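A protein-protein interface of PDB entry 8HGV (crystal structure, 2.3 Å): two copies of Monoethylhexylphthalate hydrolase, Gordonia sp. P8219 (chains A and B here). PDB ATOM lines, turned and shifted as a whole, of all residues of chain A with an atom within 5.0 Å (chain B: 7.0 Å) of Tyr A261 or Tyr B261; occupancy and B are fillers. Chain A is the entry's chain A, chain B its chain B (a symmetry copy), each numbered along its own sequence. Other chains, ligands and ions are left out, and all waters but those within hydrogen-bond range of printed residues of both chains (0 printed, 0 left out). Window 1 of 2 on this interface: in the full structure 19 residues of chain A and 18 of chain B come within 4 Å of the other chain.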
ATOM      1  N   LEU A 229      -4.734 -19.767 -11.376  1.00  0.00           N
ATOM      2  CA  LEU A 229      -3.455 -20.340 -10.984  1.00  0.00           C
ATOM      3  C   LEU A 229      -2.372 -19.279 -11.086  1.00  0.00           C
ATOM      4  O   LEU A 229      -2.331 -18.513 -12.051  1.00  0.00           O
ATOM      5  CB  LEU A 229      -3.105 -21.547 -11.859  1.00  0.00           C
ATOM      6  CG  LEU A 229      -1.708 -22.153 -11.714  1.00  0.00           C
ATOM      7  CD1 LEU A 229      -1.588 -22.930 -10.416  1.00  0.00           C
ATOM      8  CD2 LEU A 229      -1.390 -23.041 -12.905  1.00  0.00           C
ATOM      9  N   VAL A 230      -1.510 -19.221 -10.079  1.00  0.00           N
ATOM     10  CA  VAL A 230      -0.363 -18.328 -10.118  1.00  0.00           C
ATOM     11  C   VAL A 230       0.910 -19.153 -10.220  1.00  0.00           C
ATOM     12  O   VAL A 230       1.168 -20.001  -9.373  1.00  0.00           O
ATOM     13  CB  VAL A 230      -0.297 -17.424  -8.875  1.00  0.00           C
ATOM     14  CG1 VAL A 230       0.881 -16.465  -8.982  1.00  0.00           C
ATOM     15  CG2 VAL A 230      -1.603 -16.663  -8.701  1.00  0.00           C
ATOM     16  N   VAL A 231       1.693 -18.914 -11.267  1.00  0.00           N
ATOM     17  CA  VAL A 231       2.941 -19.641 -11.470  1.00  0.00           C
ATOM     18  C   VAL A 231       4.127 -18.700 -11.290  1.00  0.00           C
ATOM     19  O   VAL A 231       4.112 -17.573 -11.787  1.00  0.00           O
ATOM     20  CB  VAL A 231       3.001 -20.289 -12.870  1.00  0.00           C
ATOM     21  CG1 VAL A 231       4.316 -21.029 -13.067  1.00  0.00           C
ATOM     22  CG2 VAL A 231       1.823 -21.228 -13.068  1.00  0.00           C
ATOM     23  N   TRP A 232       5.149 -19.161 -10.576  1.00  0.00           N
ATOM     24  CA  TRP A 232       6.329 -18.338 -10.345  1.00  0.00           C
ATOM     25  C   TRP A 232       7.596 -19.184 -10.262  1.00  0.00           C
ATOM     26  O   TRP A 232       7.568 -20.302  -9.755  1.00  0.00           O
ATOM     27  CB  TRP A 232       6.156 -17.519  -9.063  1.00  0.00           C
ATOM     28  CG  TRP A 232       6.591 -16.084  -9.170  1.00  0.00           C
ATOM     29  CD1 TRP A 232       7.864 -15.600  -9.067  1.00  0.00           C
ATOM     30  CD2 TRP A 232       5.745 -14.945  -9.377  1.00  0.00           C
ATOM     31  NE1 TRP A 232       7.864 -14.233  -9.205  1.00  0.00           N
ATOM     32  CE2 TRP A 232       6.575 -13.807  -9.396  1.00  0.00           C
ATOM     33  CE3 TRP A 232       4.367 -14.779  -9.551  1.00  0.00           C
ATOM     34  CZ2 TRP A 232       6.072 -12.520  -9.581  1.00  0.00           C
ATOM     35  CZ3 TRP A 232       3.869 -13.502  -9.735  1.00  0.00           C
ATOM     36  CH2 TRP A 232       4.719 -12.388  -9.749  1.00  0.00           C
ATOM     37  N   SER A 259      -4.783 -21.196  -6.825  1.00  0.00           N
ATOM     38  CA  SER A 259      -3.644 -22.079  -6.575  1.00  0.00           C
ATOM     39  C   SER A 259      -2.317 -21.355  -6.774  1.00  0.00           C
ATOM     40  O   SER A 259      -2.244 -20.380  -7.523  1.00  0.00           O
ATOM     41  CB  SER A 259      -3.701 -23.300  -7.494  1.00  0.00           C
ATOM     42  OG  SER A 259      -4.065 -24.463  -6.781  1.00  0.00           O
ATOM     43  N   LEU A 260      -1.269 -21.833  -6.106  1.00  0.00           N
ATOM     44  CA  LEU A 260       0.068 -21.270  -6.292  1.00  0.00           C
ATOM     45  C   LEU A 260       1.103 -22.355  -6.560  1.00  0.00           C
ATOM     46  O   LEU A 260       1.240 -23.303  -5.791  1.00  0.00           O
ATOM     47  CB  LEU A 260       0.493 -20.447  -5.072  1.00  0.00           C
ATOM     48  CG  LEU A 260       1.894 -19.826  -5.162  1.00  0.00           C
ATOM     49  CD1 LEU A 260       1.961 -18.761  -6.253  1.00  0.00           C
ATOM     50  CD2 LEU A 260       2.340 -19.253  -3.821  1.00  0.00           C
ATOM     51  N   TYR A 261       1.834 -22.201  -7.656  1.00  0.00           N
ATOM     52  CA  TYR A 261       2.879 -23.140  -8.022  1.00  0.00           C
ATOM     53  C   TYR A 261       4.214 -22.416  -8.173  1.00  0.00           C
ATOM     54  O   TYR A 261       4.361 -21.520  -9.010  1.00  0.00           O
ATOM     55  CB  TYR A 261       2.511 -23.876  -9.314  1.00  0.00           C
ATOM     56  CG  TYR A 261       3.340 -25.111  -9.577  1.00  0.00           C
ATOM     57  CD1 TYR A 261       3.416 -26.130  -8.635  1.00  0.00           C
ATOM     58  CD2 TYR A 261       4.036 -25.268 -10.768  1.00  0.00           C
ATOM     59  CE1 TYR A 261       4.169 -27.265  -8.868  1.00  0.00           C
ATOM     60  CE2 TYR A 261       4.793 -26.402 -11.012  1.00  0.00           C
ATOM     61  CZ  TYR A 261       4.854 -27.396 -10.058  1.00  0.00           C
ATOM     62  OH  TYR A 261       5.604 -28.528 -10.288  1.00  0.00           O
ATOM     63  N   LEU A 262       5.178 -22.801  -7.343  1.00  0.00           N
ATOM     64  CA  LEU A 262       6.521 -22.240  -7.399  1.00  0.00           C
ATOM     65  C   LEU A 262       7.506 -23.301  -7.872  1.00  0.00           C
ATOM     66  O   LEU A 262       7.636 -24.356  -7.252  1.00  0.00           O
ATOM     67  CB  LEU A 262       6.950 -21.698  -6.030  1.00  0.00           C
ATOM     68  CG  LEU A 262       6.000 -20.748  -5.292  1.00  0.00           C
ATOM     69  CD1 LEU A 262       6.602 -20.316  -3.965  1.00  0.00           C
ATOM     70  CD2 LEU A 262       5.659 -19.537  -6.143  1.00  0.00           C
ATOM     71  N   ILE A 263       8.196 -23.022  -8.972  1.00  0.00           N
ATOM     72  CA  ILE A 263       9.188 -23.948  -9.498  1.00  0.00           C
ATOM     73  C   ILE A 263      10.595 -23.471  -9.166  1.00  0.00           C
ATOM     74  O   ILE A 263      10.953 -22.330  -9.454  1.00  0.00           O
ATOM     75  CB  ILE A 263       9.054 -24.118 -11.020  1.00  0.00           C
ATOM     76  CG1 ILE A 263       7.598 -24.405 -11.390  1.00  0.00           C
ATOM     77  CG2 ILE A 263       9.964 -25.228 -11.512  1.00  0.00           C
ATOM     78  CD1 ILE A 263       7.345 -24.483 -12.879  1.00  0.00           C
ATOM     79  N   LYS A 277       8.132 -29.371 -16.276  1.00  0.00           N
ATOM     80  CA  LYS A 277       7.354 -29.071 -15.072  1.00  0.00           C
ATOM     81  C   LYS A 277       6.213 -28.096 -15.352  1.00  0.00           C
ATOM     82  O   LYS A 277       5.063 -28.342 -14.978  1.00  0.00           O
ATOM     83  CB  LYS A 277       8.248 -28.487 -13.979  1.00  0.00           C
ATOM     84  CG  LYS A 277       9.055 -29.494 -13.188  1.00  0.00           C
ATOM     85  CD  LYS A 277       9.789 -28.793 -12.055  1.00  0.00           C
ATOM     86  CE  LYS A 277      10.597 -29.762 -11.214  1.00  0.00           C
ATOM     87  NZ  LYS A 277      11.409 -29.040 -10.188  1.00  0.00           N
ATOM     88  N   ALA A 281       2.214 -29.064 -14.893  1.00  0.00           N
ATOM     89  CA  ALA A 281       1.355 -28.424 -13.900  1.00  0.00           C
ATOM     90  C   ALA A 281       0.270 -27.564 -14.540  1.00  0.00           C
ATOM     91  O   ALA A 281      -0.918 -27.706 -14.224  1.00  0.00           O
ATOM     92  CB  ALA A 281       2.183 -27.585 -12.952  1.00  0.00           C
ATOM     93  N   THR B 228      11.360 -33.447  -5.638  1.00  0.00           N
ATOM     94  CA  THR B 228      10.448 -33.282  -4.512  1.00  0.00           C
ATOM     95  C   THR B 228       9.304 -32.311  -4.789  1.00  0.00           C
ATOM     96  O   THR B 228       9.499 -31.238  -5.371  1.00  0.00           O
ATOM     97  CB  THR B 228      11.208 -32.807  -3.253  1.00  0.00           C
ATOM     98  OG1 THR B 228      12.305 -33.693  -2.993  1.00  0.00           O
ATOM     99  CG2 THR B 228      10.284 -32.786  -2.039  1.00  0.00           C
ATOM    100  N   LEU B 229       8.107 -32.707  -4.368  1.00  0.00           N
ATOM    101  CA  LEU B 229       6.935 -31.846  -4.423  1.00  0.00           C
ATOM    102  C   LEU B 229       6.377 -31.642  -3.021  1.00  0.00           C
ATOM    103  O   LEU B 229       6.132 -32.608  -2.296  1.00  0.00           O
ATOM    104  CB  LEU B 229       5.865 -32.446  -5.342  1.00  0.00           C
ATOM    105  CG  LEU B 229       4.510 -31.734  -5.416  1.00  0.00           C
ATOM    106  CD1 LEU B 229       4.650 -30.338  -5.999  1.00  0.00           C
ATOM    107  CD2 LEU B 229       3.518 -32.554  -6.223  1.00  0.00           C
ATOM    108  N   VAL B 230       6.193 -30.386  -2.634  1.00  0.00           N
ATOM    109  CA  VAL B 230       5.544 -30.074  -1.368  1.00  0.00           C
ATOM    110  C   VAL B 230       4.134 -29.579  -1.640  1.00  0.00           C
ATOM    111  O   VAL B 230       3.942 -28.640  -2.403  1.00  0.00           O
ATOM    112  CB  VAL B 230       6.316 -29.009  -0.568  1.00  0.00           C
ATOM    113  CG1 VAL B 230       5.570 -28.663   0.713  1.00  0.00           C
ATOM    114  CG2 VAL B 230       7.721 -29.494  -0.256  1.00  0.00           C
ATOM    115  N   VAL B 231       3.145 -30.221  -1.028  1.00  0.00           N
ATOM    116  CA  VAL B 231       1.758 -29.812  -1.205  1.00  0.00           C
ATOM    117  C   VAL B 231       1.209 -29.269   0.108  1.00  0.00           C
ATOM    118  O   VAL B 231       1.435 -29.853   1.170  1.00  0.00           O
ATOM    119  CB  VAL B 231       0.882 -30.981  -1.696  1.00  0.00           C
ATOM    120  CG1 VAL B 231      -0.542 -30.508  -1.967  1.00  0.00           C
ATOM    121  CG2 VAL B 231       1.485 -31.599  -2.945  1.00  0.00           C
ATOM    122  N   TRP B 232       0.495 -28.149   0.041  1.00  0.00           N
ATOM    123  CA  TRP B 232      -0.049 -27.557   1.260  1.00  0.00           C
ATOM    124  C   TRP B 232      -1.411 -26.915   1.046  1.00  0.00           C
ATOM    125  O   TRP B 232      -1.697 -26.379  -0.027  1.00  0.00           O
ATOM    126  CB  TRP B 232       0.919 -26.516   1.820  1.00  0.00           C
ATOM    127  CG  TRP B 232       1.107 -26.599   3.300  1.00  0.00           C
ATOM    128  CD1 TRP B 232       0.291 -26.080   4.262  1.00  0.00           C
ATOM    129  CD2 TRP B 232       2.189 -27.232   3.992  1.00  0.00           C
ATOM    130  NE1 TRP B 232       0.797 -26.354   5.509  1.00  0.00           N
ATOM    131  CE2 TRP B 232       1.964 -27.061   5.370  1.00  0.00           C
ATOM    132  CE3 TRP B 232       3.329 -27.930   3.578  1.00  0.00           C
ATOM    133  CZ2 TRP B 232       2.831 -27.562   6.337  1.00  0.00           C
ATOM    134  CZ3 TRP B 232       4.190 -28.426   4.538  1.00  0.00           C
ATOM    135  CH2 TRP B 232       3.937 -28.239   5.901  1.00  0.00           C
ATOM    136  N   GLY B 233      -2.247 -26.973   2.077  1.00  0.00           N
ATOM    137  CA  GLY B 233      -3.510 -26.262   2.079  1.00  0.00           C
ATOM    138  C   GLY B 233      -3.327 -24.911   2.745  1.00  0.00           C
ATOM    139  O   GLY B 233      -2.801 -24.829   3.859  1.00  0.00           O
ATOM    140  N   PHE B 248       9.798 -25.465   2.284  1.00  0.00           N
ATOM    141  CA  PHE B 248      10.124 -25.417   0.864  1.00  0.00           C
ATOM    142  C   PHE B 248      11.344 -24.543   0.603  1.00  0.00           C
ATOM    143  O   PHE B 248      12.086 -24.797  -0.336  1.00  0.00           O
ATOM    144  CB  PHE B 248       8.949 -24.911   0.028  1.00  0.00           C
ATOM    145  CG  PHE B 248       9.284 -24.736  -1.429  1.00  0.00           C
ATOM    146  CD1 PHE B 248       9.531 -25.839  -2.231  1.00  0.00           C
ATOM    147  CD2 PHE B 248       9.367 -23.473  -1.992  1.00  0.00           C
ATOM    148  CE1 PHE B 248       9.848 -25.685  -3.568  1.00  0.00           C
ATOM    149  CE2 PHE B 248       9.683 -23.312  -3.329  1.00  0.00           C
ATOM    150  CZ  PHE B 248       9.922 -24.421  -4.119  1.00  0.00           C
ATOM    151  N   SER B 258      12.796 -29.254  -7.267  1.00  0.00           N
ATOM    152  CA  SER B 258      11.831 -29.158  -6.181  1.00  0.00           C
ATOM    153  C   SER B 258      10.722 -28.190  -6.560  1.00  0.00           C
ATOM    154  O   SER B 258      10.925 -27.294  -7.379  1.00  0.00           O
ATOM    155  CB  SER B 258      12.510 -28.716  -4.882  1.00  0.00           C
ATOM    156  OG  SER B 258      13.196 -27.489  -5.054  1.00  0.00           O
ATOM    157  N   SER B 259       9.549 -28.371  -5.966  1.00  0.00           N
ATOM    158  CA  SER B 259       8.401 -27.550  -6.322  1.00  0.00           C
ATOM    159  C   SER B 259       7.422 -27.415  -5.165  1.00  0.00           C
ATOM    160  O   SER B 259       7.303 -28.313  -4.334  1.00  0.00           O
ATOM    161  CB  SER B 259       7.695 -28.139  -7.540  1.00  0.00           C
ATOM    162  OG  SER B 259       7.266 -27.113  -8.410  1.00  0.00           O
ATOM    163  N   LEU B 260       6.718 -26.289  -5.121  1.00  0.00           N
ATOM    164  CA  LEU B 260       5.721 -26.046  -4.085  1.00  0.00           C
ATOM    165  C   LEU B 260       4.348 -25.794  -4.696  1.00  0.00           C
ATOM    166  O   LEU B 260       4.208 -25.004  -5.626  1.00  0.00           O
ATOM    167  CB  LEU B 260       6.131 -24.861  -3.210  1.00  0.00           C
ATOM    168  CG  LEU B 260       5.122 -24.430  -2.143  1.00  0.00           C
ATOM    169  CD1 LEU B 260       4.950 -25.515  -1.094  1.00  0.00           C
ATOM    170  CD2 LEU B 260       5.533 -23.114  -1.502  1.00  0.00           C
ATOM    171  N   TYR B 261       3.336 -26.474  -4.169  1.00  0.00           N
ATOM    172  CA  TYR B 261       1.968 -26.286  -4.627  1.00  0.00           C
ATOM    173  C   TYR B 261       1.057 -25.932  -3.456  1.00  0.00           C
ATOM    174  O   TYR B 261       0.848 -26.737  -2.538  1.00  0.00           O
ATOM    175  CB  TYR B 261       1.461 -27.538  -5.344  1.00  0.00           C
ATOM    176  CG  TYR B 261       0.186 -27.310  -6.119  1.00  0.00           C
ATOM    177  CD1 TYR B 261       0.089 -26.273  -7.035  1.00  0.00           C
ATOM    178  CD2 TYR B 261      -0.916 -28.131  -5.943  1.00  0.00           C
ATOM    179  CE1 TYR B 261      -1.073 -26.053  -7.749  1.00  0.00           C
ATOM    180  CE2 TYR B 261      -2.085 -27.921  -6.656  1.00  0.00           C
ATOM    181  CZ  TYR B 261      -2.156 -26.881  -7.555  1.00  0.00           C
ATOM    182  OH  TYR B 261      -3.313 -26.661  -8.267  1.00  0.00           O
ATOM    183  N   LEU B 262       0.536 -24.709  -3.488  1.00  0.00           N
ATOM    184  CA  LEU B 262      -0.388 -24.239  -2.467  1.00  0.00           C
ATOM    185  C   LEU B 262      -1.814 -24.222  -3.006  1.00  0.00           C
ATOM    186  O   LEU B 262      -2.105 -23.564  -4.008  1.00  0.00           O
ATOM    187  CB  LEU B 262       0.008 -22.845  -1.980  1.00  0.00           C
ATOM    188  CG  LEU B 262       1.396 -22.713  -1.353  1.00  0.00           C
ATOM    189  CD1 LEU B 262       1.612 -21.316  -0.801  1.00  0.00           C
ATOM    190  CD2 LEU B 262       1.584 -23.753  -0.270  1.00  0.00           C
ATOM    191  N   ILE B 263      -2.697 -24.950  -2.334  1.00  0.00           N
ATOM    192  CA  ILE B 263      -4.093 -25.034  -2.738  1.00  0.00           C
ATOM    193  C   ILE B 263      -4.970 -24.234  -1.787  1.00  0.00           C
ATOM    194  O   ILE B 263      -4.981 -24.477  -0.578  1.00  0.00           O
ATOM    195  CB  ILE B 263      -4.575 -26.495  -2.780  1.00  0.00           C
ATOM    196  CG1 ILE B 263      -3.624 -27.334  -3.636  1.00  0.00           C
ATOM    197  CG2 ILE B 263      -5.998 -26.574  -3.306  1.00  0.00           C
ATOM    198  CD1 ILE B 263      -4.048 -28.784  -3.805  1.00  0.00           C
ATOM    199  N   VAL B 270      -5.671 -31.968   2.711  1.00  0.00           N
ATOM    200  CA  VAL B 270      -5.767 -31.306   1.410  1.00  0.00           C
ATOM    201  C   VAL B 270      -6.429 -32.174   0.344  1.00  0.00           C
ATOM    202  O   VAL B 270      -7.254 -31.692  -0.435  1.00  0.00           O
ATOM    203  CB  VAL B 270      -4.375 -30.889   0.890  1.00  0.00           C
ATOM    204  CG1 VAL B 270      -4.463 -29.562   0.163  1.00  0.00           C
ATOM    205  CG2 VAL B 270      -3.381 -30.805   2.033  1.00  0.00           C
ATOM    206  N   LYS B 277      -8.061 -30.928  -7.898  1.00  0.00           N
ATOM    207  CA  LYS B 277      -6.802 -30.189  -8.015  1.00  0.00           C
ATOM    208  C   LYS B 277      -5.614 -31.002  -7.516  1.00  0.00           C
ATOM    209  O   LYS B 277      -4.557 -31.040  -8.155  1.00  0.00           O
ATOM    210  CB  LYS B 277      -6.862 -28.878  -7.234  1.00  0.00           C
ATOM    211  CG  LYS B 277      -7.628 -27.761  -7.900  1.00  0.00           C
ATOM    212  CD  LYS B 277      -7.228 -26.435  -7.277  1.00  0.00           C
ATOM    213  CE  LYS B 277      -8.115 -25.309  -7.751  1.00  0.00           C
ATOM    214  NZ  LYS B 277      -7.728 -24.012  -7.133  1.00  0.00           N
ATOM    215  N   PHE B 278      -5.795 -31.631  -6.359  1.00  0.00           N
ATOM    216  CA  PHE B 278      -4.756 -32.446  -5.743  1.00  0.00           C
ATOM    217  C   PHE B 278      -4.312 -33.552  -6.692  1.00  0.00           C
ATOM    218  O   PHE B 278      -3.125 -33.684  -6.996  1.00  0.00           O
ATOM    219  CB  PHE B 278      -5.260 -33.037  -4.424  1.00  0.00           C
ATOM    220  CG  PHE B 278      -4.279 -33.952  -3.756  1.00  0.00           C
ATOM    221  CD1 PHE B 278      -3.287 -33.444  -2.934  1.00  0.00           C
ATOM    222  CD2 PHE B 278      -4.352 -35.322  -3.943  1.00  0.00           C
ATOM    223  CE1 PHE B 278      -2.379 -34.285  -2.318  1.00  0.00           C
ATOM    224  CE2 PHE B 278      -3.449 -36.167  -3.329  1.00  0.00           C
ATOM    225  CZ  PHE B 278      -2.461 -35.647  -2.515  1.00  0.00           C
ATOM    226  N   ALA B 280      -4.821 -33.791  -9.903  1.00  0.00           N
ATOM    227  CA  ALA B 280      -4.266 -33.220 -11.127  1.00  0.00           C
ATOM    228  C   ALA B 280      -2.785 -32.875 -10.968  1.00  0.00           C
ATOM    229  O   ALA B 280      -1.946 -33.301 -11.769  1.00  0.00           O
ATOM    230  CB  ALA B 280      -5.056 -31.985 -11.543  1.00  0.00           C
ATOM    231  N   ALA B 281      -2.471 -32.114  -9.923  1.00  0.00           N
ATOM    232  CA  ALA B 281      -1.101 -31.660  -9.694  1.00  0.00           C
ATOM    233  C   ALA B 281      -0.153 -32.801  -9.326  1.00  0.00           C
ATOM    234  O   ALA B 281       0.894 -32.979  -9.958  1.00  0.00           O
ATOM    235  CB  ALA B 281      -1.077 -30.600  -8.612  1.00  0.00           C
ATOM    236  N   VAL B 282      -0.512 -33.565  -8.297  1.00  0.00           N
ATOM    237  CA  VAL B 282       0.347 -34.650  -7.835  1.00  0.00           C
ATOM    238  C   VAL B 282       0.513 -35.707  -8.924  1.00  0.00           C
ATOM    239  O   VAL B 282       1.606 -36.241  -9.120  1.00  0.00           O
ATOM    240  CB  VAL B 282      -0.205 -35.298  -6.551  1.00  0.00           C
ATOM    241  CG1 VAL B 282       0.669 -36.472  -6.125  1.00  0.00           C
ATOM    242  CG2 VAL B 282      -0.296 -34.262  -5.438  1.00  0.00           C
ATOM    243  N   PHE B 285       2.961 -34.449 -11.395  1.00  0.00           N
ATOM    244  CA  PHE B 285       4.311 -34.617 -10.865  1.00  0.00           C
ATOM    245  C   PHE B 285       4.809 -36.056 -11.000  1.00  0.00           C
ATOM    246  O   PHE B 285       5.960 -36.289 -11.376  1.00  0.00           O
ATOM    247  CB  PHE B 285       4.358 -34.186  -9.396  1.00  0.00           C
ATOM    248  CG  PHE B 285       5.698 -34.394  -8.739  1.00  0.00           C
ATOM    249  CD1 PHE B 285       6.781 -33.594  -9.070  1.00  0.00           C
ATOM    250  CD2 PHE B 285       5.865 -35.373  -7.771  1.00  0.00           C
ATOM    251  CE1 PHE B 285       8.007 -33.776  -8.461  1.00  0.00           C
ATOM    252  CE2 PHE B 285       7.090 -35.559  -7.157  1.00  0.00           C
ATOM    253  CZ  PHE B 285       8.162 -34.760  -7.503  1.00  0.00           C
ATOM    254  N   LEU B 288       5.915 -37.287 -14.586  1.00  0.00           N
ATOM    255  CA  LEU B 288       7.111 -36.697 -15.187  1.00  0.00           C
ATOM    256  C   LEU B 288       8.152 -37.764 -15.523  1.00  0.00           C
ATOM    257  O   LEU B 288       9.093 -37.514 -16.284  1.00  0.00           O
ATOM    258  CB  LEU B 288       7.732 -35.650 -14.259  1.00  0.00           C
ATOM    259  CG  LEU B 288       7.117 -34.249 -14.206  1.00  0.00           C
ATOM    260  CD1 LEU B 288       7.935 -33.349 -13.292  1.00  0.00           C
ATOM    261  CD2 LEU B 288       7.024 -33.651 -15.595  1.00  0.00           C
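Ser A259 touches Tyr B261, and with the chains exchanged Tyr A261 touches Ser B259.
Ser A259 touches Leu B262, and with the chains exchanged Leu A262 touches Ser B259.
Leu A260 touches Leu B262, and with the chains exchanged Leu A262 touches Leu B260.
Ile A263 touches Ser B259, but with the chains exchanged Ser A259 does not touch Ile B263 (4.1 Å).
Of the 14 pairs that touch across the chains among the printed residues, 10 have their exchanged pair printed and touching as well.
O of Leu B262 touches CA of Ser A259 (3.3 Å).
Ser A259 touches Lys B277 (OG to NZ, 3.7 Å).
CA of Tyr B261 touches O of Leu A260, at 3.3 Å.
CD1 of Tyr A261 touches O of Leu B260 (3.3 Å).
Tyr A261 touches Tyr B261 (CD1 to CD1, 3.7 Å).
O of Leu A262 touches CZ of Phe B248, at 3.9 Å.
Ser B259 touches Ile A263 (OG to CA, 3.9 Å).
Tyr A261 touches three residues of chain B.
Printed residues of chain B within 4 Å of Leu A262: Phe B248, Ser B259 and Leu B260.
Of the printed residues of chain B, Ile A263 touches Ser B259 (3.9 Å).
Of the printed residues of chain B, Lys A277 touches Ser B258 (3.2 Å).
Tyr B261 touches three residues of chain A.
The nearest residue of chain B that does not touch Tyr A261 is Leu B229 (4.2 Å).
O of Tyr A261 is in hydrogen-bond range of N of Trp A232 (2.9 Å).
The backbone NH of Ile A263 is in hydrogen-bond range of the backbone carbonyl oxygen of Trp A232 (2.9 Å).
The backbone carbonyl oxygen of Val A230 lies within hydrogen-bond range of the backbone NH of Tyr A261 (2.9 Å).
N of Ser B259 lies within hydrogen-bond range of O of Thr B228.
The backbone NH (N) of Tyr B261 sits at hydrogen-bond distance from the backbone carbonyl oxygen (O) of Val B230, 2.9 Å away.
The backbone NH (N) of Trp B232 is in hydrogen-bond range of the backbone carbonyl oxygen (O) of Tyr B261, 3.0 Å away.
The backbone carbonyl oxygen of Leu A260 lies close to the backbone carbonyl oxygen of Leu B260, at 3.4 Å.
OH of Tyr B261 sits at hydrogen-bond distance from OG of Ser A259 (2.8 Å).
The side-chain hydroxyl (OH) of Tyr A261 lies within hydrogen-bond range of the side-chain hydroxyl (OG) of Ser B259, at 2.9 Å.
O of Leu A260 is in hydrogen-bond range of N of Leu B262, 2.8 Å away.
NZ of Lys A277 lies within hydrogen-bond range of O of Ser B258, 3.3 Å away.
The backbone NH (N) of Leu A262 sits at hydrogen-bond distance from the backbone carbonyl oxygen (O) of Leu B260, at 3.0 Å.
The backbone carbonyl oxygen (O) of Leu A262 sits at hydrogen-bond distance from the side-chain hydroxyl (OG) of Ser B259 (3.0 Å).
Of the 21 printed residues of chain B, 7 touch a printed residue of chain A.
Printed residues of chain B that touch a printed residue of chain A: Phe B248, Ser B258, Ser B259, Leu B260, Tyr B261, Leu B262 and Lys B277.
Hydrophobic or aromatic side chains of chain B that line the printed part of chain A: Phe B248, Leu B260, Tyr B261 and Leu B262.
Among the printed residues, 14 pairs touch across the chains.
Among the printed residues, no Asp or Glu carboxylate lies within 4 Å of a Lys or Arg side-chain nitrogen of the other chain.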
